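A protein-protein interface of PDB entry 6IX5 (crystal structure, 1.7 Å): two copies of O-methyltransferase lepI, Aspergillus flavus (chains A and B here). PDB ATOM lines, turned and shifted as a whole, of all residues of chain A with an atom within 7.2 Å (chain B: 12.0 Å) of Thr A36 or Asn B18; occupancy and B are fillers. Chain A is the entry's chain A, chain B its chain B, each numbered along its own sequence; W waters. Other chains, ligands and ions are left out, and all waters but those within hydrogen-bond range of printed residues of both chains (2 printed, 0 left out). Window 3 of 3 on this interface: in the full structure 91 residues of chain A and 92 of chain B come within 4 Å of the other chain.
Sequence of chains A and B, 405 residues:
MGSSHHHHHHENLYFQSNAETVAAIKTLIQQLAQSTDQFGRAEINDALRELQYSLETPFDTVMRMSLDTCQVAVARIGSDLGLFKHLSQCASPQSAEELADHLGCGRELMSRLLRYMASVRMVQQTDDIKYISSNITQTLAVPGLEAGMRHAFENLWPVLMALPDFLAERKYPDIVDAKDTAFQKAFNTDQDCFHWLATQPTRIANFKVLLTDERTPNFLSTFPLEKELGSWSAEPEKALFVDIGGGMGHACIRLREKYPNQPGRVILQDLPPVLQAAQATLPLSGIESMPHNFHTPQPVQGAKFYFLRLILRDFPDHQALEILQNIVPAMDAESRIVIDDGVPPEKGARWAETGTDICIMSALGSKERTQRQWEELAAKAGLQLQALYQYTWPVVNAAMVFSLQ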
ATOM      1  N   GLN A  31      13.274 -19.154  -2.743  1.00  0.00           N
ATOM      2  CA  GLN A  31      14.292 -18.995  -1.713  1.00  0.00           C
ATOM      3  C   GLN A  31      13.730 -19.276  -0.334  1.00  0.00           C
ATOM      4  O   GLN A  31      14.419 -19.886   0.497  1.00  0.00           O
ATOM      5  CB  GLN A  31      14.880 -17.590  -1.773  1.00  0.00           C
ATOM      6  CG  GLN A  31      15.667 -17.403  -3.053  1.00  0.00           C
ATOM      7  CD  GLN A  31      16.832 -18.401  -3.140  1.00  0.00           C
ATOM      8  OE1 GLN A  31      16.983 -19.137  -4.138  1.00  0.00           O
ATOM      9  NE2 GLN A  31      17.650 -18.435  -2.098  1.00  0.00           N
ATOM     10  N   LEU A  32      12.494 -18.825  -0.050  1.00  0.00           N
ATOM     11  CA  LEU A  32      11.919 -19.129   1.265  1.00  0.00           C
ATOM     12  C   LEU A  32      11.706 -20.630   1.415  1.00  0.00           C
ATOM     13  O   LEU A  32      11.908 -21.202   2.495  1.00  0.00           O
ATOM     14  CB  LEU A  32      10.597 -18.371   1.461  1.00  0.00           C
ATOM     15  CG  LEU A  32      10.760 -16.854   1.559  1.00  0.00           C
ATOM     16  CD1 LEU A  32       9.414 -16.178   1.314  1.00  0.00           C
ATOM     17  CD2 LEU A  32      11.302 -16.459   2.920  1.00  0.00           C
ATOM     18  N   ALA A  33      11.277 -21.284   0.336  1.00  0.00           N
ATOM     19  CA  ALA A  33      11.046 -22.730   0.391  1.00  0.00           C
ATOM     20  C   ALA A  33      12.339 -23.487   0.659  1.00  0.00           C
ATOM     21  O   ALA A  33      12.343 -24.440   1.443  1.00  0.00           O
ATOM     22  CB  ALA A  33      10.420 -23.188  -0.915  1.00  0.00           C
ATOM     23  N   GLN A  34      13.446 -23.074   0.039  1.00  0.00           N
ATOM     24  CA  GLN A  34      14.722 -23.742   0.313  1.00  0.00           C
ATOM     25  C   GLN A  34      15.233 -23.494   1.725  1.00  0.00           C
ATOM     26  O   GLN A  34      15.974 -24.338   2.250  1.00  0.00           O
ATOM     27  CB  GLN A  34      15.795 -23.306  -0.689  1.00  0.00           C
ATOM     28  CG  GLN A  34      15.483 -23.747  -2.094  1.00  0.00           C
ATOM     29  CD  GLN A  34      16.377 -23.102  -3.152  1.00  0.00           C
ATOM     30  OE1 GLN A  34      17.455 -22.576  -2.838  1.00  0.00           O
ATOM     31  NE2 GLN A  34      15.936 -23.151  -4.420  1.00  0.00           N
ATOM     32  N   SER A  35      14.836 -22.396   2.369  1.00  0.00           N
ATOM     33  CA  SER A  35      15.311 -22.074   3.719  1.00  0.00           C
ATOM     34  C   SER A  35      14.547 -22.794   4.817  1.00  0.00           C
ATOM     35  O   SER A  35      14.856 -22.582   5.992  1.00  0.00           O
ATOM     36  CB  SER A  35      15.217 -20.564   3.985  1.00  0.00           C
ATOM     37  OG  SER A  35      13.857 -20.153   4.205  1.00  0.00           O
ATOM     38  N   THR A  36      13.546 -23.609   4.486  1.00  0.00           N
ATOM     39  CA  THR A  36      12.792 -24.308   5.515  1.00  0.00           C
ATOM     40  C   THR A  36      12.903 -25.805   5.224  1.00  0.00           C
ATOM     41  O   THR A  36      13.712 -26.232   4.388  1.00  0.00           O
ATOM     42  CB  THR A  36      11.347 -23.794   5.589  1.00  0.00           C
ATOM     43  OG1 THR A  36      10.664 -24.416   6.700  1.00  0.00           O
ATOM     44  CG2 THR A  36      10.577 -24.062   4.281  1.00  0.00           C
ATOM     45  N   ASP A  37      12.133 -26.604   5.942  1.00  0.00           N
ATOM     46  CA  ASP A  37      12.197 -28.047   5.770  1.00  0.00           C
ATOM     47  C   ASP A  37      10.962 -28.506   5.022  1.00  0.00           C
ATOM     48  O   ASP A  37      10.171 -27.685   4.527  1.00  0.00           O
ATOM     49  CB  ASP A  37      12.353 -28.752   7.125  1.00  0.00           C
ATOM     50  CG  ASP A  37      11.197 -28.472   8.083  1.00  0.00           C
ATOM     51  OD1 ASP A  37      10.174 -27.870   7.690  1.00  0.00           O
ATOM     52  OD2 ASP A  37      11.311 -28.860   9.257  1.00  0.00           O
ATOM     53  N   GLN A  38      10.759 -29.829   4.936  1.00  0.00           N
ATOM     54  CA  GLN A  38       9.659 -30.284   4.090  1.00  0.00           C
ATOM     55  C   GLN A  38       8.313 -29.890   4.678  1.00  0.00           C
ATOM     56  O   GLN A  38       7.345 -29.681   3.931  1.00  0.00           O
ATOM     57  CB  GLN A  38       9.748 -31.800   3.868  1.00  0.00           C
ATOM     58  CG  GLN A  38       9.673 -32.578   5.120  1.00  0.00           C
ATOM     59  CD  GLN A  38       9.722 -34.081   4.906  1.00  0.00           C
ATOM     60  OE1 GLN A  38      10.411 -34.781   5.653  1.00  0.00           O
ATOM     61  NE2 GLN A  38       8.979 -34.593   3.895  1.00  0.00           N
ATOM     62  N   PHE A  39       8.229 -29.744   6.000  1.00  0.00           N
ATOM     63  CA  PHE A  39       6.940 -29.388   6.582  1.00  0.00           C
ATOM     64  C   PHE A  39       6.621 -27.923   6.305  1.00  0.00           C
ATOM     65  O   PHE A  39       5.477 -27.580   5.974  1.00  0.00           O
ATOM     66  CB  PHE A  39       6.941 -29.693   8.084  1.00  0.00           C
ATOM     67  CG  PHE A  39       7.366 -31.099   8.398  1.00  0.00           C
ATOM     68  CD1 PHE A  39       6.751 -32.172   7.774  1.00  0.00           C
ATOM     69  CD2 PHE A  39       8.425 -31.342   9.270  1.00  0.00           C
ATOM     70  CE1 PHE A  39       7.142 -33.470   8.022  1.00  0.00           C
ATOM     71  CE2 PHE A  39       8.835 -32.683   9.543  1.00  0.00           C
ATOM     72  CZ  PHE A  39       8.191 -33.738   8.926  1.00  0.00           C
ATOM     73  N   GLY A  40       7.633 -27.064   6.406  1.00  0.00           N
ATOM     74  CA  GLY A  40       7.465 -25.664   6.034  1.00  0.00           C
ATOM     75  C   GLY A  40       7.142 -25.485   4.557  1.00  0.00           C
ATOM     76  O   GLY A  40       6.352 -24.609   4.191  1.00  0.00           O
ATOM     77  N   ARG A  41       7.736 -26.312   3.688  1.00  0.00           N
ATOM     78  CA  ARG A  41       7.359 -26.227   2.269  1.00  0.00           C
ATOM     79  C   ARG A  41       5.923 -26.669   2.043  1.00  0.00           C
ATOM     80  O   ARG A  41       5.226 -26.126   1.168  1.00  0.00           O
ATOM     81  CB  ARG A  41       8.284 -27.053   1.373  1.00  0.00           C
ATOM     82  CG  ARG A  41       9.608 -26.378   1.154  1.00  0.00           C
ATOM     83  CD  ARG A  41      10.518 -27.119   0.179  1.00  0.00           C
ATOM     84  NE  ARG A  41      11.035 -28.349   0.780  1.00  0.00           N
ATOM     85  CZ  ARG A  41      12.096 -28.398   1.583  1.00  0.00           C
ATOM     86  NH1 ARG A  41      12.495 -29.565   2.099  1.00  0.00           N
ATOM     87  NH2 ARG A  41      12.741 -27.279   1.891  1.00  0.00           N
ATOM     88  N   ALA A  42       5.479 -27.689   2.764  1.00  0.00           N
ATOM     89  CA  ALA A  42       4.085 -28.083   2.649  1.00  0.00           C
ATOM     90  C   ALA A  42       3.164 -26.958   3.100  1.00  0.00           C
ATOM     91  O   ALA A  42       2.109 -26.753   2.498  1.00  0.00           O
ATOM     92  CB  ALA A  42       3.823 -29.358   3.459  1.00  0.00           C
ATOM     93  N   GLU A  43       3.535 -26.224   4.169  1.00  0.00           N
ATOM     94  CA  GLU A  43       2.718 -25.084   4.584  1.00  0.00           C
ATOM     95  C   GLU A  43       2.712 -23.981   3.522  1.00  0.00           C
ATOM     96  O   GLU A  43       1.664 -23.377   3.253  1.00  0.00           O
ATOM     97  CB  GLU A  43       3.214 -24.511   5.906  1.00  0.00           C
ATOM     98  CG  GLU A  43       2.870 -25.387   7.075  1.00  0.00           C
ATOM     99  CD  GLU A  43       3.248 -24.690   8.368  1.00  0.00           C
ATOM    100  OE1 GLU A  43       2.616 -23.640   8.692  1.00  0.00           O
ATOM    101  OE2 GLU A  43       4.208 -25.166   9.018  1.00  0.00           O
ATOM    102  N   ILE A  44       3.868 -23.703   2.908  1.00  0.00           N
ATOM    103  CA  ILE A  44       3.912 -22.698   1.854  1.00  0.00           C
ATOM    104  C   ILE A  44       3.024 -23.125   0.695  1.00  0.00           C
ATOM    105  O   ILE A  44       2.244 -22.326   0.167  1.00  0.00           O
ATOM    106  CB  ILE A  44       5.365 -22.457   1.391  1.00  0.00           C
ATOM    107  CG1 ILE A  44       6.165 -21.786   2.499  1.00  0.00           C
ATOM    108  CG2 ILE A  44       5.403 -21.633   0.050  1.00  0.00           C
ATOM    109  CD1 ILE A  44       7.680 -21.812   2.224  1.00  0.00           C
ATOM    110  N   TRP A 393       3.391 -32.932   9.276  1.00  0.00           N
ATOM    111  CA  TRP A 393       2.717 -31.648   9.447  1.00  0.00           C
ATOM    112  C   TRP A 393       2.705 -30.983   8.079  1.00  0.00           C
ATOM    113  O   TRP A 393       3.640 -31.170   7.301  1.00  0.00           O
ATOM    114  CB  TRP A 393       3.447 -30.705  10.426  1.00  0.00           C
ATOM    115  CG  TRP A 393       3.650 -31.222  11.773  1.00  0.00           C
ATOM    116  CD1 TRP A 393       2.867 -30.959  12.867  1.00  0.00           C
ATOM    117  CD2 TRP A 393       4.711 -32.090  12.228  1.00  0.00           C
ATOM    118  NE1 TRP A 393       3.361 -31.627  13.954  1.00  0.00           N
ATOM    119  CE2 TRP A 393       4.488 -32.326  13.601  1.00  0.00           C
ATOM    120  CE3 TRP A 393       5.804 -32.702  11.601  1.00  0.00           C
ATOM    121  CZ2 TRP A 393       5.323 -33.151  14.373  1.00  0.00           C
ATOM    122  CZ3 TRP A 393       6.651 -33.502  12.367  1.00  0.00           C
ATOM    123  CH2 TRP A 393       6.395 -33.726  13.740  1.00  0.00           C
ATOM    124  N   SER B  17       9.257 -18.427  12.552  1.00  0.00           N
ATOM    125  CA  SER B  17       8.033 -19.234  12.597  1.00  0.00           C
ATOM    126  C   SER B  17       7.449 -19.452  11.193  1.00  0.00           C
ATOM    127  O   SER B  17       7.360 -18.500  10.377  1.00  0.00           O
ATOM    128  CB  SER B  17       6.995 -18.566  13.516  1.00  0.00           C
ATOM    129  OG  SER B  17       5.650 -18.804  13.096  1.00  0.00           O
ATOM    130  N   ASN B  18       7.070 -20.710  10.912  1.00  0.00           N
ATOM    131  CA  ASN B  18       6.423 -21.059   9.646  1.00  0.00           C
ATOM    132  C   ASN B  18       5.120 -20.304   9.468  1.00  0.00           C
ATOM    133  O   ASN B  18       4.820 -19.784   8.386  1.00  0.00           O
ATOM    134  CB  ASN B  18       6.121 -22.557   9.602  1.00  0.00           C
ATOM    135  CG  ASN B  18       7.357 -23.405   9.501  1.00  0.00           C
ATOM    136  OD1 ASN B  18       8.479 -22.884   9.477  1.00  0.00           O
ATOM    137  ND2 ASN B  18       7.162 -24.734   9.441  1.00  0.00           N
ATOM    138  N   ALA B  19       4.289 -20.308  10.509  1.00  0.00           N
ATOM    139  CA  ALA B  19       3.022 -19.601  10.396  1.00  0.00           C
ATOM    140  C   ALA B  19       3.252 -18.118  10.098  1.00  0.00           C
ATOM    141  O   ALA B  19       2.562 -17.543   9.263  1.00  0.00           O
ATOM    142  CB  ALA B  19       2.191 -19.794  11.662  1.00  0.00           C
ATOM    143  N   GLU B  20       4.241 -17.494  10.747  1.00  0.00           N
ATOM    144  CA  GLU B  20       4.510 -16.078  10.478  1.00  0.00           C
ATOM    145  C   GLU B  20       4.960 -15.867   9.030  1.00  0.00           C
ATOM    146  O   GLU B  20       4.532 -14.904   8.361  1.00  0.00           O
ATOM    147  CB  GLU B  20       5.564 -15.553  11.466  1.00  0.00           C
ATOM    148  CG  GLU B  20       5.801 -14.032  11.445  1.00  0.00           C
ATOM    149  CD  GLU B  20       7.009 -13.580  12.315  1.00  0.00           C
ATOM    150  OE1 GLU B  20       7.341 -14.295  13.290  1.00  0.00           O
ATOM    151  OE2 GLU B  20       7.635 -12.520  11.998  1.00  0.00           O
ATOM    152  N   THR B  21       5.855 -16.726   8.538  1.00  0.00           N
ATOM    153  CA  THR B  21       6.300 -16.619   7.146  1.00  0.00           C
ATOM    154  C   THR B  21       5.144 -16.787   6.178  1.00  0.00           C
ATOM    155  O   THR B  21       5.021 -16.025   5.215  1.00  0.00           O
ATOM    156  CB  THR B  21       7.400 -17.647   6.861  1.00  0.00           C
ATOM    157  OG1 THR B  21       8.525 -17.325   7.678  1.00  0.00           O
ATOM    158  CG2 THR B  21       7.828 -17.607   5.384  1.00  0.00           C
ATOM    159  N   VAL B  22       4.301 -17.807   6.394  1.00  0.00           N
ATOM    160  CA  VAL B  22       3.191 -18.051   5.480  1.00  0.00           C
ATOM    161  C   VAL B  22       2.231 -16.865   5.466  1.00  0.00           C
ATOM    162  O   VAL B  22       1.759 -16.431   4.401  1.00  0.00           O
ATOM    163  CB  VAL B  22       2.485 -19.363   5.867  1.00  0.00           C
ATOM    164  CG1 VAL B  22       1.061 -19.371   5.412  1.00  0.00           C
ATOM    165  CG2 VAL B  22       3.287 -20.553   5.327  1.00  0.00           C
ATOM    166  N   ALA B  23       1.978 -16.276   6.634  1.00  0.00           N
ATOM    167  CA  ALA B  23       1.053 -15.156   6.668  1.00  0.00           C
ATOM    168  C   ALA B  23       1.662 -13.972   5.965  1.00  0.00           C
ATOM    169  O   ALA B  23       0.932 -13.203   5.322  1.00  0.00           O
ATOM    170  CB  ALA B  23       0.683 -14.766   8.114  1.00  0.00           C
ATOM    171  N   ALA B  24       2.995 -13.835   6.046  1.00  0.00           N
ATOM    172  CA  ALA B  24       3.641 -12.707   5.381  1.00  0.00           C
ATOM    173  C   ALA B  24       3.617 -12.882   3.859  1.00  0.00           C
ATOM    174  O   ALA B  24       3.427 -11.916   3.110  1.00  0.00           O
ATOM    175  CB  ALA B  24       5.082 -12.528   5.867  1.00  0.00           C
ATOM    176  N   ILE B  25       3.799 -14.122   3.382  1.00  0.00           N
ATOM    177  CA  ILE B  25       3.658 -14.361   1.946  1.00  0.00           C
ATOM    178  C   ILE B  25       2.262 -13.981   1.467  1.00  0.00           C
ATOM    179  O   ILE B  25       2.102 -13.341   0.415  1.00  0.00           O
ATOM    180  CB  ILE B  25       3.960 -15.837   1.635  1.00  0.00           C
ATOM    181  CG1 ILE B  25       5.433 -16.117   1.889  1.00  0.00           C
ATOM    182  CG2 ILE B  25       3.450 -16.242   0.205  1.00  0.00           C
ATOM    183  CD1 ILE B  25       5.762 -17.648   1.853  1.00  0.00           C
ATOM    184  N   LYS B  26       1.231 -14.425   2.200  1.00  0.00           N
ATOM    185  CA  LYS B  26      -0.141 -14.099   1.835  1.00  0.00           C
ATOM    186  C   LYS B  26      -0.368 -12.593   1.782  1.00  0.00           C
ATOM    187  O   LYS B  26      -0.992 -12.082   0.841  1.00  0.00           O
ATOM    188  CB  LYS B  26      -1.110 -14.751   2.830  1.00  0.00           C
ATOM    189  CG  LYS B  26      -1.129 -16.290   2.703  1.00  0.00           C
ATOM    190  CD  LYS B  26      -2.288 -16.811   3.561  1.00  0.00           C
ATOM    191  CE  LYS B  26      -2.210 -18.316   3.704  1.00  0.00           C
ATOM    192  NZ  LYS B  26      -3.147 -18.839   4.725  1.00  0.00           N
ATOM    193  N   THR B  27       0.118 -11.862   2.801  1.00  0.00           N
ATOM    194  CA  THR B  27      -0.072 -10.409   2.825  1.00  0.00           C
ATOM    195  C   THR B  27       0.583  -9.771   1.609  1.00  0.00           C
ATOM    196  O   THR B  27      -0.001  -8.901   0.939  1.00  0.00           O
ATOM    197  CB  THR B  27       0.533  -9.811   4.123  1.00  0.00           C
ATOM    198  OG1 THR B  27      -0.174 -10.316   5.279  1.00  0.00           O
ATOM    199  CG2 THR B  27       0.487  -8.251   4.113  1.00  0.00           C
ATOM    200  N   LEU B  51       4.617 -22.459  -9.101  1.00  0.00           N
ATOM    201  CA  LEU B  51       5.382 -22.618  -7.856  1.00  0.00           C
ATOM    202  C   LEU B  51       4.923 -23.838  -7.075  1.00  0.00           C
ATOM    203  O   LEU B  51       5.749 -24.633  -6.611  1.00  0.00           O
ATOM    204  CB  LEU B  51       5.252 -21.381  -6.977  1.00  0.00           C
ATOM    205  CG  LEU B  51       6.151 -20.232  -7.388  1.00  0.00           C
ATOM    206  CD1 LEU B  51       5.614 -18.950  -6.712  1.00  0.00           C
ATOM    207  CD2 LEU B  51       7.620 -20.492  -7.048  1.00  0.00           C
ATOM    208  N   LEU B  55       7.324 -27.094  -6.126  1.00  0.00           N
ATOM    209  CA  LEU B  55       7.709 -27.264  -4.721  1.00  0.00           C
ATOM    210  C   LEU B  55       7.101 -28.511  -4.063  1.00  0.00           C
ATOM    211  O   LEU B  55       7.587 -28.924  -3.014  1.00  0.00           O
ATOM    212  CB  LEU B  55       7.315 -26.023  -3.913  1.00  0.00           C
ATOM    213  CG  LEU B  55       8.234 -24.860  -4.361  1.00  0.00           C
ATOM    214  CD1 LEU B  55       7.770 -23.549  -3.784  1.00  0.00           C
ATOM    215  CD2 LEU B  55       9.746 -25.123  -4.016  1.00  0.00           C
ATOM    216  N   GLU B  56       6.110 -29.150  -4.692  1.00  0.00           N
ATOM    217  CA  GLU B  56       5.477 -30.322  -4.100  1.00  0.00           C
ATOM    218  C   GLU B  56       6.417 -31.529  -4.140  1.00  0.00           C
ATOM    219  O   GLU B  56       7.283 -31.653  -5.019  1.00  0.00           O
ATOM    220  CB  GLU B  56       4.172 -30.651  -4.842  1.00  0.00           C
ATOM    221  CG  GLU B  56       4.402 -31.182  -6.209  1.00  0.00           C
ATOM    222  CD  GLU B  56       3.144 -31.148  -7.090  1.00  0.00           C
ATOM    223  OE1 GLU B  56       2.083 -30.741  -6.584  1.00  0.00           O
ATOM    224  OE2 GLU B  56       3.232 -31.530  -8.278  1.00  0.00           O
ATOM    225  N   THR B  57       6.263 -32.415  -3.149  1.00  0.00           N
ATOM    226  CA  THR B  57       7.030 -33.661  -3.179  1.00  0.00           C
ATOM    227  C   THR B  57       6.415 -34.609  -4.196  1.00  0.00           C
ATOM    228  O   THR B  57       5.270 -34.420  -4.615  1.00  0.00           O
ATOM    229  CB  THR B  57       7.028 -34.370  -1.837  1.00  0.00           C
ATOM    230  OG1 THR B  57       5.682 -34.738  -1.488  1.00  0.00           O
ATOM    231  CG2 THR B  57       7.579 -33.454  -0.728  1.00  0.00           C
ATOM    232  N   ASP B  60       3.168 -35.738  -2.911  1.00  0.00           N
ATOM    233  CA  ASP B  60       2.175 -34.669  -2.985  1.00  0.00           C
ATOM    234  C   ASP B  60       1.618 -34.527  -4.390  1.00  0.00           C
ATOM    235  O   ASP B  60       0.437 -34.206  -4.557  1.00  0.00           O
ATOM    236  CB  ASP B  60       2.752 -33.299  -2.583  1.00  0.00           C
ATOM    237  CG  ASP B  60       3.075 -33.154  -1.131  1.00  0.00           C
ATOM    238  OD1 ASP B  60       2.537 -33.889  -0.274  1.00  0.00           O
ATOM    239  OD2 ASP B  60       3.909 -32.244  -0.850  1.00  0.00           O
HETATM  240  O   HOH W   1       8.745 -26.752   9.499  1.00  0.00           O
HETATM  241  O   HOH W   2      11.173 -23.446   9.245  1.00  0.00           O
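No position is printed for both chains.
Of the 15 printed residues of chain A, 5 touch a printed residue of chain B. Printed residues of chain A that touch a printed residue of chain B: Leu A32, Ala A33, Thr A36, Gly A40 and Glu A43. Hydrophobic or aromatic side chains of chain A that line the printed part of chain B: Leu A32 and Ala A33. Along chain B the printed residues that touch a printed residue of chain A span positions 18 to 55. Among the printed residues, 6 pairs touch across the chains. Among the printed residues, no Asp or Glu carboxylate lies within 4 Å of a Lys or Arg side-chain nitrogen of the other chain.
NH2 of Arg A41 sits at hydrogen-bond distance from O of Ala A33 (2.9 Å). The backbone carbonyl oxygen (O) of Leu A32 sits at hydrogen-bond distance from the side-chain hydroxyl (OG) of Ser A35. O of Thr A36 sits at hydrogen-bond distance from NH2 of Arg A41 (2.9 Å). OD1 of Asp A37 lies within hydrogen-bond range of N of Gly A40 (3.0 Å).
Ile B25 touches Leu A32. Ala A33 touches Leu B55. Thr A36 touches Asn B18 (OG1 to OD1, 3.9 Å). Asn B18 touches Gly A40 (ND2 to CA, 3.5 Å). Glu A43 touches Val B22 (O to CG2, 3.9 Å).
Of the printed residues of chain A, Asn B18 touches Thr A36, Gly A40 and Glu A43. Of chain B, only Leu B55 comes within 4 Å of Ala A33. Ser A35 touches none of the printed residues of chain B. Asp A37 touches none of the printed residues of chain B. Of the printed residues of chain B, Leu A32 touches Ile B25. Of the printed residues of chain A, Ile B25 touches Leu A32 (3.97 Å). Of the printed residues of chain A, Leu B55 touches Ala A33. Of the printed residues of chain B, Gly A40 touches Asn B18 (3.5 Å). Gln A38 touches none of the printed residues of chain B. The nearest printed residue of chain A that does not touch Asn B18 is Phe A39 (4.5 Å).
Water W1 lies within hydrogen-bond range of the side-chain carboxylate (OD1) of Asp A37 (2.6 Å), the side-chain amide nitrogen (ND2) of Asn B18 (2.6 Å) and the backbone NH (N) of Gly A40 (3.3 Å). Water W2 bridges OD1 of Asn B18 (2.8 Å) and OG1 of Thr A36 (2.8 Å).
OE2 of Glu A43 sits at hydrogen-bond distance from ND2 of Asn B18.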
